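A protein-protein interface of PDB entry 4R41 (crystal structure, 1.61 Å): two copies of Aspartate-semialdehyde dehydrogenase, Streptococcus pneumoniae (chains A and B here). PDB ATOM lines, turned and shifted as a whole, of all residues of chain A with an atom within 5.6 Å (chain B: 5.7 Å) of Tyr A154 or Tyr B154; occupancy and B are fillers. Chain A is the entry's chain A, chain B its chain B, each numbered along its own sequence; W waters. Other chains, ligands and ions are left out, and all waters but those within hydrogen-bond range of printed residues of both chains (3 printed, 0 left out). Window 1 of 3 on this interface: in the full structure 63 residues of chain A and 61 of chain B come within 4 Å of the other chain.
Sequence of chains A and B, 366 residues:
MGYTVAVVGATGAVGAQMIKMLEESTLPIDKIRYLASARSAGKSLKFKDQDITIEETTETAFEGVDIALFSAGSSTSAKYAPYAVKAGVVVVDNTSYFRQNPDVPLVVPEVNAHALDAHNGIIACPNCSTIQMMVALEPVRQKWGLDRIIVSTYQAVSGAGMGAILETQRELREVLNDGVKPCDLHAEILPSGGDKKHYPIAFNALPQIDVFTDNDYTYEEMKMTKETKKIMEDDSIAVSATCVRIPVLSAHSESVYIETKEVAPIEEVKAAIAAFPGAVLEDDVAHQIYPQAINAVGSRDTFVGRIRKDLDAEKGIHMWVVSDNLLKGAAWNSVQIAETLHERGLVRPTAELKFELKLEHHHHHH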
ATOM      1  N   SER A 152     -18.028 -25.217 -28.001  1.00  0.00           N
ATOM      2  CA  SER A 152     -16.633 -25.635 -27.896  1.00  0.00           C
ATOM      3  C   SER A 152     -16.027 -24.830 -26.764  1.00  0.00           C
ATOM      4  O   SER A 152     -16.102 -23.586 -26.778  1.00  0.00           O
ATOM      5  CB  SER A 152     -15.886 -25.344 -29.192  1.00  0.00           C
ATOM      6  OG  SER A 152     -16.314 -26.249 -30.197  1.00  0.00           O
ATOM      7  N   THR A 153     -15.510 -25.515 -25.747  1.00  0.00           N
ATOM      8  CA  THR A 153     -14.973 -24.787 -24.589  1.00  0.00           C
ATOM      9  C   THR A 153     -13.449 -24.661 -24.564  1.00  0.00           C
ATOM     10  O   THR A 153     -12.714 -25.444 -25.203  1.00  0.00           O
ATOM     11  CB  THR A 153     -15.414 -25.396 -23.243  1.00  0.00           C
ATOM     12  OG1 THR A 153     -14.666 -26.582 -23.007  1.00  0.00           O
ATOM     13  CG2 THR A 153     -16.949 -25.727 -23.204  1.00  0.00           C
ATOM     14  N   TYR A 154     -12.999 -23.676 -23.787  1.00  0.00           N
ATOM     15  CA  TYR A 154     -11.582 -23.317 -23.648  1.00  0.00           C
ATOM     16  C   TYR A 154     -11.383 -23.156 -22.152  1.00  0.00           C
ATOM     17  O   TYR A 154     -11.489 -22.046 -21.614  1.00  0.00           O
ATOM     18  CB  TYR A 154     -11.278 -21.987 -24.357  1.00  0.00           C
ATOM     19  CG  TYR A 154     -11.526 -21.958 -25.867  1.00  0.00           C
ATOM     20  CD1 TYR A 154     -12.828 -22.039 -26.404  1.00  0.00           C
ATOM     21  CD2 TYR A 154     -10.467 -21.778 -26.750  1.00  0.00           C
ATOM     22  CE1 TYR A 154     -13.048 -21.995 -27.783  1.00  0.00           C
ATOM     23  CE2 TYR A 154     -10.688 -21.735 -28.142  1.00  0.00           C
ATOM     24  CZ  TYR A 154     -11.980 -21.852 -28.645  1.00  0.00           C
ATOM     25  OH  TYR A 154     -12.192 -21.795 -30.014  1.00  0.00           O
ATOM     26  N   GLN A 155     -11.150 -24.279 -21.477  1.00  0.00           N
ATOM     27  CA  GLN A 155     -11.293 -24.321 -20.020  1.00  0.00           C
ATOM     28  C   GLN A 155      -9.982 -24.196 -19.271  1.00  0.00           C
ATOM     29  O   GLN A 155      -8.968 -24.790 -19.658  1.00  0.00           O
ATOM     30  CB  GLN A 155     -12.039 -25.587 -19.592  1.00  0.00           C
ATOM     31  CG  GLN A 155     -13.527 -25.491 -19.942  1.00  0.00           C
ATOM     32  CD  GLN A 155     -14.307 -26.742 -19.625  1.00  0.00           C
ATOM     33  OE1 GLN A 155     -14.952 -27.309 -20.524  1.00  0.00           O
ATOM     34  NE2 GLN A 155     -14.286 -27.180 -18.348  1.00  0.00           N
ATOM     35  N   ALA A 156     -10.027 -23.391 -18.213  1.00  0.00           N
ATOM     36  CA  ALA A 156      -8.899 -23.187 -17.300  1.00  0.00           C
ATOM     37  C   ALA A 156      -8.636 -24.420 -16.396  1.00  0.00           C
ATOM     38  O   ALA A 156      -9.534 -25.254 -16.141  1.00  0.00           O
ATOM     39  CB  ALA A 156      -9.122 -21.918 -16.471  1.00  0.00           C
ATOM     40  N   ALA A 205      -3.391 -28.126 -26.047  1.00  0.00           N
ATOM     41  CA  ALA A 205      -4.857 -28.025 -25.949  1.00  0.00           C
ATOM     42  C   ALA A 205      -5.373 -29.437 -25.855  1.00  0.00           C
ATOM     43  O   ALA A 205      -5.210 -30.215 -26.792  1.00  0.00           O
ATOM     44  CB  ALA A 205      -5.433 -27.292 -27.161  1.00  0.00           C
ATOM     45  N   THR A 242     -17.944 -29.883 -27.106  1.00  0.00           N
ATOM     46  CA  THR A 242     -16.566 -30.363 -27.108  1.00  0.00           C
ATOM     47  C   THR A 242     -15.852 -29.582 -26.011  1.00  0.00           C
ATOM     48  O   THR A 242     -15.881 -28.358 -26.046  1.00  0.00           O
ATOM     49  CB  THR A 242     -15.866 -30.075 -28.454  1.00  0.00           C
ATOM     50  OG1 THR A 242     -16.582 -30.710 -29.517  1.00  0.00           O
ATOM     51  CG2 THR A 242     -14.386 -30.560 -28.454  1.00  0.00           C
ATOM     52  N   VAL A 244     -12.466 -28.602 -23.929  1.00  0.00           N
ATOM     53  CA  VAL A 244     -11.017 -28.645 -24.159  1.00  0.00           C
ATOM     54  C   VAL A 244     -10.324 -27.862 -23.033  1.00  0.00           C
ATOM     55  O   VAL A 244     -10.746 -26.746 -22.699  1.00  0.00           O
ATOM     56  CB  VAL A 244     -10.664 -28.015 -25.534  1.00  0.00           C
ATOM     57  CG1 VAL A 244      -9.163 -28.088 -25.798  1.00  0.00           C
ATOM     58  CG2 VAL A 244     -11.490 -28.683 -26.658  1.00  0.00           C
ATOM     59  N   ARG A 245      -9.293 -28.465 -22.451  1.00  0.00           N
ATOM     60  CA  ARG A 245      -8.453 -27.758 -21.468  1.00  0.00           C
ATOM     61  C   ARG A 245      -7.344 -27.011 -22.203  1.00  0.00           C
ATOM     62  O   ARG A 245      -6.684 -27.563 -23.114  1.00  0.00           O
ATOM     63  CB  ARG A 245      -7.864 -28.758 -20.471  1.00  0.00           C
ATOM     64  CG  ARG A 245      -7.250 -28.117 -19.224  1.00  0.00           C
ATOM     65  CD  ARG A 245      -8.311 -27.804 -18.181  1.00  0.00           C
ATOM     66  NE  ARG A 245      -8.865 -29.044 -17.602  1.00  0.00           N
ATOM     67  CZ  ARG A 245      -9.823 -29.074 -16.685  1.00  0.00           C
ATOM     68  NH1 ARG A 245     -10.340 -27.941 -16.215  1.00  0.00           N
ATOM     69  NH2 ARG A 245     -10.262 -30.238 -16.223  1.00  0.00           N
ATOM     70  N   ILE A 246      -7.132 -25.751 -21.813  1.00  0.00           N
ATOM     71  CA  ILE A 246      -6.070 -24.928 -22.380  1.00  0.00           C
ATOM     72  C   ILE A 246      -5.185 -24.382 -21.239  1.00  0.00           C
ATOM     73  O   ILE A 246      -5.568 -24.496 -20.097  1.00  0.00           O
ATOM     74  CB  ILE A 246      -6.604 -23.807 -23.302  1.00  0.00           C
ATOM     75  CG1 ILE A 246      -7.524 -22.821 -22.550  1.00  0.00           C
ATOM     76  CG2 ILE A 246      -7.290 -24.401 -24.544  1.00  0.00           C
ATOM     77  CD1 ILE A 246      -7.677 -21.493 -23.301  1.00  0.00           C
ATOM     78  N   ALA A 251     -10.659 -18.840 -15.311  1.00  0.00           N
ATOM     79  CA  ALA A 251     -11.692 -18.276 -16.179  1.00  0.00           C
ATOM     80  C   ALA A 251     -11.842 -19.150 -17.425  1.00  0.00           C
ATOM     81  O   ALA A 251     -10.882 -19.376 -18.156  1.00  0.00           O
ATOM     82  CB  ALA A 251     -11.427 -16.816 -16.556  1.00  0.00           C
ATOM     83  N   HIS A 252     -13.047 -19.671 -17.609  1.00  0.00           N
ATOM     84  CA  HIS A 252     -13.374 -20.466 -18.790  1.00  0.00           C
ATOM     85  C   HIS A 252     -13.887 -19.589 -19.906  1.00  0.00           C
ATOM     86  O   HIS A 252     -14.575 -18.595 -19.646  1.00  0.00           O
ATOM     87  CB  HIS A 252     -14.484 -21.458 -18.460  1.00  0.00           C
ATOM     88  CG  HIS A 252     -14.079 -22.575 -17.546  1.00  0.00           C
ATOM     89  ND1 HIS A 252     -12.767 -22.907 -17.273  1.00  0.00           N
ATOM     90  CD2 HIS A 252     -14.846 -23.453 -16.844  1.00  0.00           C
ATOM     91  CE1 HIS A 252     -12.744 -23.954 -16.457  1.00  0.00           C
ATOM     92  NE2 HIS A 252     -13.992 -24.307 -16.190  1.00  0.00           N
ATOM     93  N   SER A 253     -13.590 -19.970 -21.152  1.00  0.00           N
ATOM     94  CA  SER A 253     -14.150 -19.287 -22.301  1.00  0.00           C
ATOM     95  C   SER A 253     -14.894 -20.293 -23.159  1.00  0.00           C
ATOM     96  O   SER A 253     -14.529 -21.468 -23.199  1.00  0.00           O
ATOM     97  CB  SER A 253     -13.056 -18.608 -23.136  1.00  0.00           C
ATOM     98  OG  SER A 253     -12.248 -17.754 -22.350  1.00  0.00           O
ATOM     99  N   GLU A 254     -15.930 -19.838 -23.862  1.00  0.00           N
ATOM    100  CA  GLU A 254     -16.743 -20.757 -24.675  1.00  0.00           C
ATOM    101  C   GLU A 254     -17.147 -20.094 -25.972  1.00  0.00           C
ATOM    102  O   GLU A 254     -17.616 -18.967 -25.969  1.00  0.00           O
ATOM    103  CB  GLU A 254     -18.021 -21.195 -23.930  1.00  0.00           C
ATOM    104  CG  GLU A 254     -17.731 -21.873 -22.596  1.00  0.00           C
ATOM    105  CD  GLU A 254     -18.948 -22.014 -21.708  1.00  0.00           C
ATOM    106  OE1 GLU A 254     -19.921 -21.264 -21.896  1.00  0.00           O
ATOM    107  OE2 GLU A 254     -18.918 -22.887 -20.801  1.00  0.00           O
ATOM    108  N   SER A 255     -16.944 -20.819 -27.074  1.00  0.00           N
ATOM    109  CA  SER A 255     -17.465 -20.448 -28.373  1.00  0.00           C
ATOM    110  C   SER A 255     -18.812 -21.148 -28.485  1.00  0.00           C
ATOM    111  O   SER A 255     -18.891 -22.395 -28.468  1.00  0.00           O
ATOM    112  CB  SER A 255     -16.500 -20.887 -29.494  1.00  0.00           C
ATOM    113  OG  SER A 255     -17.102 -20.615 -30.751  1.00  0.00           O
ATOM    114  N   TRP A 320     -19.277 -15.459 -27.770  1.00  0.00           N
ATOM    115  CA  TRP A 320     -18.102 -15.802 -26.962  1.00  0.00           C
ATOM    116  C   TRP A 320     -18.477 -15.446 -25.525  1.00  0.00           C
ATOM    117  O   TRP A 320     -18.849 -14.277 -25.226  1.00  0.00           O
ATOM    118  CB  TRP A 320     -16.929 -14.954 -27.435  1.00  0.00           C
ATOM    119  CG  TRP A 320     -15.576 -15.193 -26.744  1.00  0.00           C
ATOM    120  CD1 TRP A 320     -14.892 -14.327 -25.925  1.00  0.00           C
ATOM    121  CD2 TRP A 320     -14.762 -16.362 -26.869  1.00  0.00           C
ATOM    122  NE1 TRP A 320     -13.671 -14.893 -25.543  1.00  0.00           N
ATOM    123  CE2 TRP A 320     -13.579 -16.145 -26.100  1.00  0.00           C
ATOM    124  CE3 TRP A 320     -14.920 -17.586 -27.550  1.00  0.00           C
ATOM    125  CZ2 TRP A 320     -12.544 -17.101 -26.014  1.00  0.00           C
ATOM    126  CZ3 TRP A 320     -13.892 -18.565 -27.448  1.00  0.00           C
ATOM    127  CH2 TRP A 320     -12.712 -18.308 -26.694  1.00  0.00           C
ATOM    128  N   SER B 152     -14.607 -23.893 -34.470  1.00  0.00           N
ATOM    129  CA  SER B 152     -13.992 -23.030 -33.464  1.00  0.00           C
ATOM    130  C   SER B 152     -12.515 -23.404 -33.392  1.00  0.00           C
ATOM    131  O   SER B 152     -12.186 -24.576 -33.217  1.00  0.00           O
ATOM    132  CB  SER B 152     -14.685 -23.225 -32.092  1.00  0.00           C
ATOM    133  OG  SER B 152     -16.049 -22.776 -32.165  1.00  0.00           O
ATOM    134  N   THR B 153     -11.622 -22.435 -33.598  1.00  0.00           N
ATOM    135  CA  THR B 153     -10.202 -22.778 -33.658  1.00  0.00           C
ATOM    136  C   THR B 153      -9.473 -22.447 -32.342  1.00  0.00           C
ATOM    137  O   THR B 153      -9.924 -21.638 -31.537  1.00  0.00           O
ATOM    138  CB  THR B 153      -9.473 -22.060 -34.796  1.00  0.00           C
ATOM    139  OG1 THR B 153      -9.340 -20.680 -34.456  1.00  0.00           O
ATOM    140  CG2 THR B 153     -10.210 -22.214 -36.137  1.00  0.00           C
ATOM    141  N   TYR B 154      -8.310 -23.071 -32.169  1.00  0.00           N
ATOM    142  CA  TYR B 154      -7.490 -22.932 -30.969  1.00  0.00           C
ATOM    143  C   TYR B 154      -6.124 -22.709 -31.570  1.00  0.00           C
ATOM    144  O   TYR B 154      -5.346 -23.655 -31.763  1.00  0.00           O
ATOM    145  CB  TYR B 154      -7.519 -24.232 -30.144  1.00  0.00           C
ATOM    146  CG  TYR B 154      -8.869 -24.594 -29.549  1.00  0.00           C
ATOM    147  CD1 TYR B 154      -9.958 -24.934 -30.372  1.00  0.00           C
ATOM    148  CD2 TYR B 154      -9.044 -24.665 -28.155  1.00  0.00           C
ATOM    149  CE1 TYR B 154     -11.199 -25.249 -29.832  1.00  0.00           C
ATOM    150  CE2 TYR B 154     -10.290 -25.007 -27.607  1.00  0.00           C
ATOM    151  CZ  TYR B 154     -11.363 -25.292 -28.462  1.00  0.00           C
ATOM    152  OH  TYR B 154     -12.607 -25.639 -27.950  1.00  0.00           O
ATOM    153  N   GLN B 155      -5.831 -21.456 -31.936  1.00  0.00           N
ATOM    154  CA  GLN B 155      -4.666 -21.202 -32.769  1.00  0.00           C
ATOM    155  C   GLN B 155      -3.422 -20.798 -32.001  1.00  0.00           C
ATOM    156  O   GLN B 155      -3.475 -19.974 -31.091  1.00  0.00           O
ATOM    157  CB  GLN B 155      -4.969 -20.195 -33.888  1.00  0.00           C
ATOM    158  CG  GLN B 155      -5.890 -20.791 -34.964  1.00  0.00           C
ATOM    159  CD  GLN B 155      -6.337 -19.797 -36.021  1.00  0.00           C
ATOM    160  OE1 GLN B 155      -7.545 -19.549 -36.188  1.00  0.00           O
ATOM    161  NE2 GLN B 155      -5.384 -19.244 -36.770  1.00  0.00           N
ATOM    162  N   ALA B 156      -2.300 -21.361 -32.442  1.00  0.00           N
ATOM    163  CA  ALA B 156      -0.962 -21.078 -31.906  1.00  0.00           C
ATOM    164  C   ALA B 156      -0.467 -19.688 -32.338  1.00  0.00           C
ATOM    165  O   ALA B 156      -0.834 -19.179 -33.412  1.00  0.00           O
ATOM    166  CB  ALA B 156       0.011 -22.147 -32.403  1.00  0.00           C
ATOM    167  N   ALA B 205      -7.309 -16.282 -23.725  1.00  0.00           N
ATOM    168  CA  ALA B 205      -7.753 -16.774 -25.004  1.00  0.00           C
ATOM    169  C   ALA B 205      -8.365 -15.599 -25.720  1.00  0.00           C
ATOM    170  O   ALA B 205      -9.376 -15.059 -25.255  1.00  0.00           O
ATOM    171  CB  ALA B 205      -8.746 -17.912 -24.850  1.00  0.00           C
ATOM    172  N   THR B 242     -15.256 -19.262 -35.754  1.00  0.00           N
ATOM    173  CA  THR B 242     -14.780 -18.413 -34.655  1.00  0.00           C
ATOM    174  C   THR B 242     -13.317 -18.757 -34.485  1.00  0.00           C
ATOM    175  O   THR B 242     -12.986 -19.928 -34.250  1.00  0.00           O
ATOM    176  CB  THR B 242     -15.494 -18.726 -33.319  1.00  0.00           C
ATOM    177  OG1 THR B 242     -16.920 -18.534 -33.479  1.00  0.00           O
ATOM    178  CG2 THR B 242     -14.999 -17.814 -32.188  1.00  0.00           C
ATOM    179  N   VAL B 244      -9.758 -18.249 -32.530  1.00  0.00           N
ATOM    180  CA  VAL B 244      -9.287 -17.826 -31.206  1.00  0.00           C
ATOM    181  C   VAL B 244      -7.802 -18.133 -31.075  1.00  0.00           C
ATOM    182  O   VAL B 244      -7.365 -19.235 -31.423  1.00  0.00           O
ATOM    183  CB  VAL B 244     -10.046 -18.574 -30.068  1.00  0.00           C
ATOM    184  CG1 VAL B 244      -9.600 -18.106 -28.689  1.00  0.00           C
ATOM    185  CG2 VAL B 244     -11.577 -18.435 -30.215  1.00  0.00           C
ATOM    186  N   ARG B 245      -7.038 -17.168 -30.557  1.00  0.00           N
ATOM    187  CA  ARG B 245      -5.611 -17.401 -30.289  1.00  0.00           C
ATOM    188  C   ARG B 245      -5.489 -17.902 -28.842  1.00  0.00           C
ATOM    189  O   ARG B 245      -6.124 -17.340 -27.931  1.00  0.00           O
ATOM    190  CB  ARG B 245      -4.834 -16.080 -30.418  1.00  0.00           C
ATOM    191  CG  ARG B 245      -3.307 -16.242 -30.420  1.00  0.00           C
ATOM    192  CD  ARG B 245      -2.835 -16.705 -31.789  1.00  0.00           C
ATOM    193  NE  ARG B 245      -3.005 -15.663 -32.811  1.00  0.00           N
ATOM    194  CZ  ARG B 245      -2.729 -15.830 -34.097  1.00  0.00           C
ATOM    195  NH1 ARG B 245      -2.287 -17.008 -34.534  1.00  0.00           N
ATOM    196  NH2 ARG B 245      -2.928 -14.830 -34.951  1.00  0.00           N
ATOM    197  N   ILE B 246      -4.691 -18.954 -28.632  1.00  0.00           N
ATOM    198  CA  ILE B 246      -4.431 -19.470 -27.283  1.00  0.00           C
ATOM    199  C   ILE B 246      -2.910 -19.546 -27.056  1.00  0.00           C
ATOM    200  O   ILE B 246      -2.156 -19.367 -28.015  1.00  0.00           O
ATOM    201  CB  ILE B 246      -5.096 -20.853 -27.026  1.00  0.00           C
ATOM    202  CG1 ILE B 246      -4.593 -21.929 -27.995  1.00  0.00           C
ATOM    203  CG2 ILE B 246      -6.622 -20.741 -27.032  1.00  0.00           C
ATOM    204  CD1 ILE B 246      -5.014 -23.319 -27.528  1.00  0.00           C
ATOM    205  N   ALA B 251       1.331 -25.272 -33.676  1.00  0.00           N
ATOM    206  CA  ALA B 251       0.266 -26.247 -33.960  1.00  0.00           C
ATOM    207  C   ALA B 251      -1.120 -25.710 -33.603  1.00  0.00           C
ATOM    208  O   ALA B 251      -1.350 -25.344 -32.459  1.00  0.00           O
ATOM    209  CB  ALA B 251       0.531 -27.600 -33.304  1.00  0.00           C
ATOM    210  N   HIS B 252      -2.015 -25.688 -34.602  1.00  0.00           N
ATOM    211  CA  HIS B 252      -3.387 -25.198 -34.449  1.00  0.00           C
ATOM    212  C   HIS B 252      -4.254 -26.410 -34.171  1.00  0.00           C
ATOM    213  O   HIS B 252      -4.025 -27.503 -34.741  1.00  0.00           O
ATOM    214  CB  HIS B 252      -3.898 -24.554 -35.744  1.00  0.00           C
ATOM    215  CG  HIS B 252      -3.269 -23.233 -36.088  1.00  0.00           C
ATOM    216  ND1 HIS B 252      -2.499 -22.495 -35.207  1.00  0.00           N
ATOM    217  CD2 HIS B 252      -3.332 -22.504 -37.233  1.00  0.00           C
ATOM    218  CE1 HIS B 252      -2.105 -21.380 -35.795  1.00  0.00           C
ATOM    219  NE2 HIS B 252      -2.609 -21.351 -37.020  1.00  0.00           N
ATOM    220  N   SER B 253      -5.260 -26.216 -33.324  1.00  0.00           N
ATOM    221  CA  SER B 253      -6.261 -27.244 -33.098  1.00  0.00           C
ATOM    222  C   SER B 253      -7.629 -26.660 -33.482  1.00  0.00           C
ATOM    223  O   SER B 253      -7.859 -25.451 -33.374  1.00  0.00           O
ATOM    224  CB  SER B 253      -6.266 -27.645 -31.621  1.00  0.00           C
ATOM    225  OG  SER B 253      -4.950 -27.938 -31.148  1.00  0.00           O
ATOM    226  N   GLU B 254      -8.533 -27.518 -33.925  1.00  0.00           N
ATOM    227  CA  GLU B 254      -9.856 -27.051 -34.362  1.00  0.00           C
ATOM    228  C   GLU B 254     -10.913 -28.017 -33.917  1.00  0.00           C
ATOM    229  O   GLU B 254     -10.792 -29.211 -34.110  1.00  0.00           O
ATOM    230  CB  GLU B 254      -9.923 -26.911 -35.895  1.00  0.00           C
ATOM    231  CG  GLU B 254      -8.886 -25.955 -36.451  1.00  0.00           C
ATOM    232  CD  GLU B 254      -8.817 -25.980 -37.966  1.00  0.00           C
ATOM    233  OE1 GLU B 254      -9.220 -26.980 -38.569  1.00  0.00           O
ATOM    234  OE2 GLU B 254      -8.301 -25.013 -38.541  1.00  0.00           O
ATOM    235  N   SER B 255     -11.966 -27.474 -33.310  1.00  0.00           N
ATOM    236  CA  SER B 255     -13.140 -28.238 -33.018  1.00  0.00           C
ATOM    237  C   SER B 255     -14.083 -28.033 -34.216  1.00  0.00           C
ATOM    238  O   SER B 255     -14.585 -26.931 -34.444  1.00  0.00           O
ATOM    239  CB  SER B 255     -13.777 -27.710 -31.727  1.00  0.00           C
ATOM    240  OG  SER B 255     -14.997 -28.365 -31.451  1.00  0.00           O
ATOM    241  N   TRP B 320     -11.932 -33.345 -33.961  1.00  0.00           N
ATOM    242  CA  TRP B 320     -10.844 -32.518 -33.427  1.00  0.00           C
ATOM    243  C   TRP B 320      -9.671 -32.675 -34.396  1.00  0.00           C
ATOM    244  O   TRP B 320      -9.264 -33.809 -34.674  1.00  0.00           O
ATOM    245  CB  TRP B 320     -10.441 -33.048 -32.049  1.00  0.00           C
ATOM    246  CG  TRP B 320      -9.324 -32.257 -31.315  1.00  0.00           C
ATOM    247  CD1 TRP B 320      -8.040 -32.695 -31.030  1.00  0.00           C
ATOM    248  CD2 TRP B 320      -9.431 -30.953 -30.745  1.00  0.00           C
ATOM    249  NE1 TRP B 320      -7.365 -31.742 -30.319  1.00  0.00           N
ATOM    250  CE2 TRP B 320      -8.185 -30.655 -30.134  1.00  0.00           C
ATOM    251  CE3 TRP B 320     -10.457 -29.993 -30.701  1.00  0.00           C
ATOM    252  CZ2 TRP B 320      -7.944 -29.448 -29.456  1.00  0.00           C
ATOM    253  CZ3 TRP B 320     -10.210 -28.765 -30.059  1.00  0.00           C
ATOM    254  CH2 TRP B 320      -8.955 -28.501 -29.442  1.00  0.00           C
HETATM  255  O   HOH W   1     -17.672 -24.861 -32.015  1.00  0.00           O
HETATM  256  O   HOH W   2      -4.443 -30.187 -29.438  1.00  0.00           O
HETATM  257  O   HOH W   3     -11.230 -15.306 -23.196  1.00  0.00           O
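OG of Ser B255 sits at hydrogen-bond distance from OG of Ser A152, at 2.8 Å.
The backbone carbonyl oxygen of Thr A153 is in hydrogen-bond range of the side-chain hydroxyl of Tyr B154 (2.8 Å).
The side-chain hydroxyl (OH) of Tyr A154 sits at hydrogen-bond distance from the backbone carbonyl oxygen (O) of Thr B153, 2.7 Å away.
OG1 of Thr A242 lies within hydrogen-bond range of OG of Ser B255, 3.4 Å away.
OG of Ser A255 is in hydrogen-bond range of OG of Ser B152 (2.8 Å).
The side-chain hydroxyl (OG) of Ser A255 lies within hydrogen-bond range of the side-chain hydroxyl (OG1) of Thr B242.
OG1 of Thr A153 lies within hydrogen-bond range of OE1 of Gln A155 (2.6 Å).
OG1 of Thr A153 sits at hydrogen-bond distance from N of Val A244 (3.1 Å).
The backbone NH of Tyr A154 lies within hydrogen-bond range of the backbone carbonyl oxygen of Ser A253, at 2.7 Å.
The backbone NH (N) of Ile A246 sits at hydrogen-bond distance from the backbone carbonyl oxygen (O) of Gln A155.
The side-chain hydroxyl of Thr B153 is in hydrogen-bond range of the side-chain amide oxygen of Gln B155 (2.7 Å).
O of Thr B242 is in hydrogen-bond range of N of Thr B153.
Among the printed residues, merely in contact across the chains: Ser A152 with Ser B152, Ser A152 with Tyr B154, Tyr A154 with Ser B152, Tyr A154 with Tyr B154, Tyr A154 with Val B244, Tyr A154 with Ile B246, Ala A205 with Trp B320, Val A244 with Tyr B154, Val A244 with Trp B320, Ile A246 with Ile B246, Trp A320 with Ala B205 and Trp A320 with Val B244.
Of the printed residues of chain B, Tyr A154 touches Ser B152 (3.5 Å), Thr B153 (2.7 Å), Tyr B154 (3.3 Å), Val B244 (3.4 Å) and Ile B246 (3.99 Å).
Tyr B154 touches just these residues of chain A: Ser A152, Thr A153, Tyr A154 and Val A244.
Of the printed residues of chain A, Ser B152 touches Ser A152, Tyr A154 and Ser A255.
Of the printed residues of chain A, Trp B320 touches Ala A205 (3.9 Å) and Val A244 (3.6 Å).
Printed residues of chain A within 4 Å of Ala B205: Trp A320 (3.8 Å).
The nearest printed residue of chain B that does not touch Tyr A154 is Ala B205 (4.6 Å).
Hydrophobic or aromatic side chains of chain A that line the printed part of chain B: Tyr A154, Val A244, Ile A246 and Trp A320.
Among the printed residues, 18 pairs touch across the chains.
Among the printed residues, no Asp or Glu carboxylate lies within 4 Å of a Lys or Arg side-chain nitrogen of the other chain.
Tyr A154 touches its own counterpart, Tyr B154.
Tyr A154 touches Ile B246, but with the chains exchanged Ile A246 does not touch Tyr B154 (4.02 Å).
Thr A242 touches Ser B255, and with the chains exchanged Ser A255 touches Thr B242.
Val A244 touches Trp B320, and with the chains exchanged Trp A320 touches Val B244.
16 positions are printed for both chains.
Of the 18 pairs that touch across the chains among the printed residues, 17 have their exchanged pair printed and touching as well.
Water W1 lies within hydrogen-bond range of OG of Ser B152 (2.6 Å) and OG of Ser A152 (2.7 Å).
Water W2 lies within hydrogen-bond range of the backbone carbonyl oxygen of Ala A205 (2.8 Å), the side-chain hydroxyl of Ser B253 (2.9 Å) and the indole nitrogen of Trp B320 (3.4 Å).
Water W3 lies within hydrogen-bond range of O of Ala B205, OG of Ser A253 and NE1 of Trp A320.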
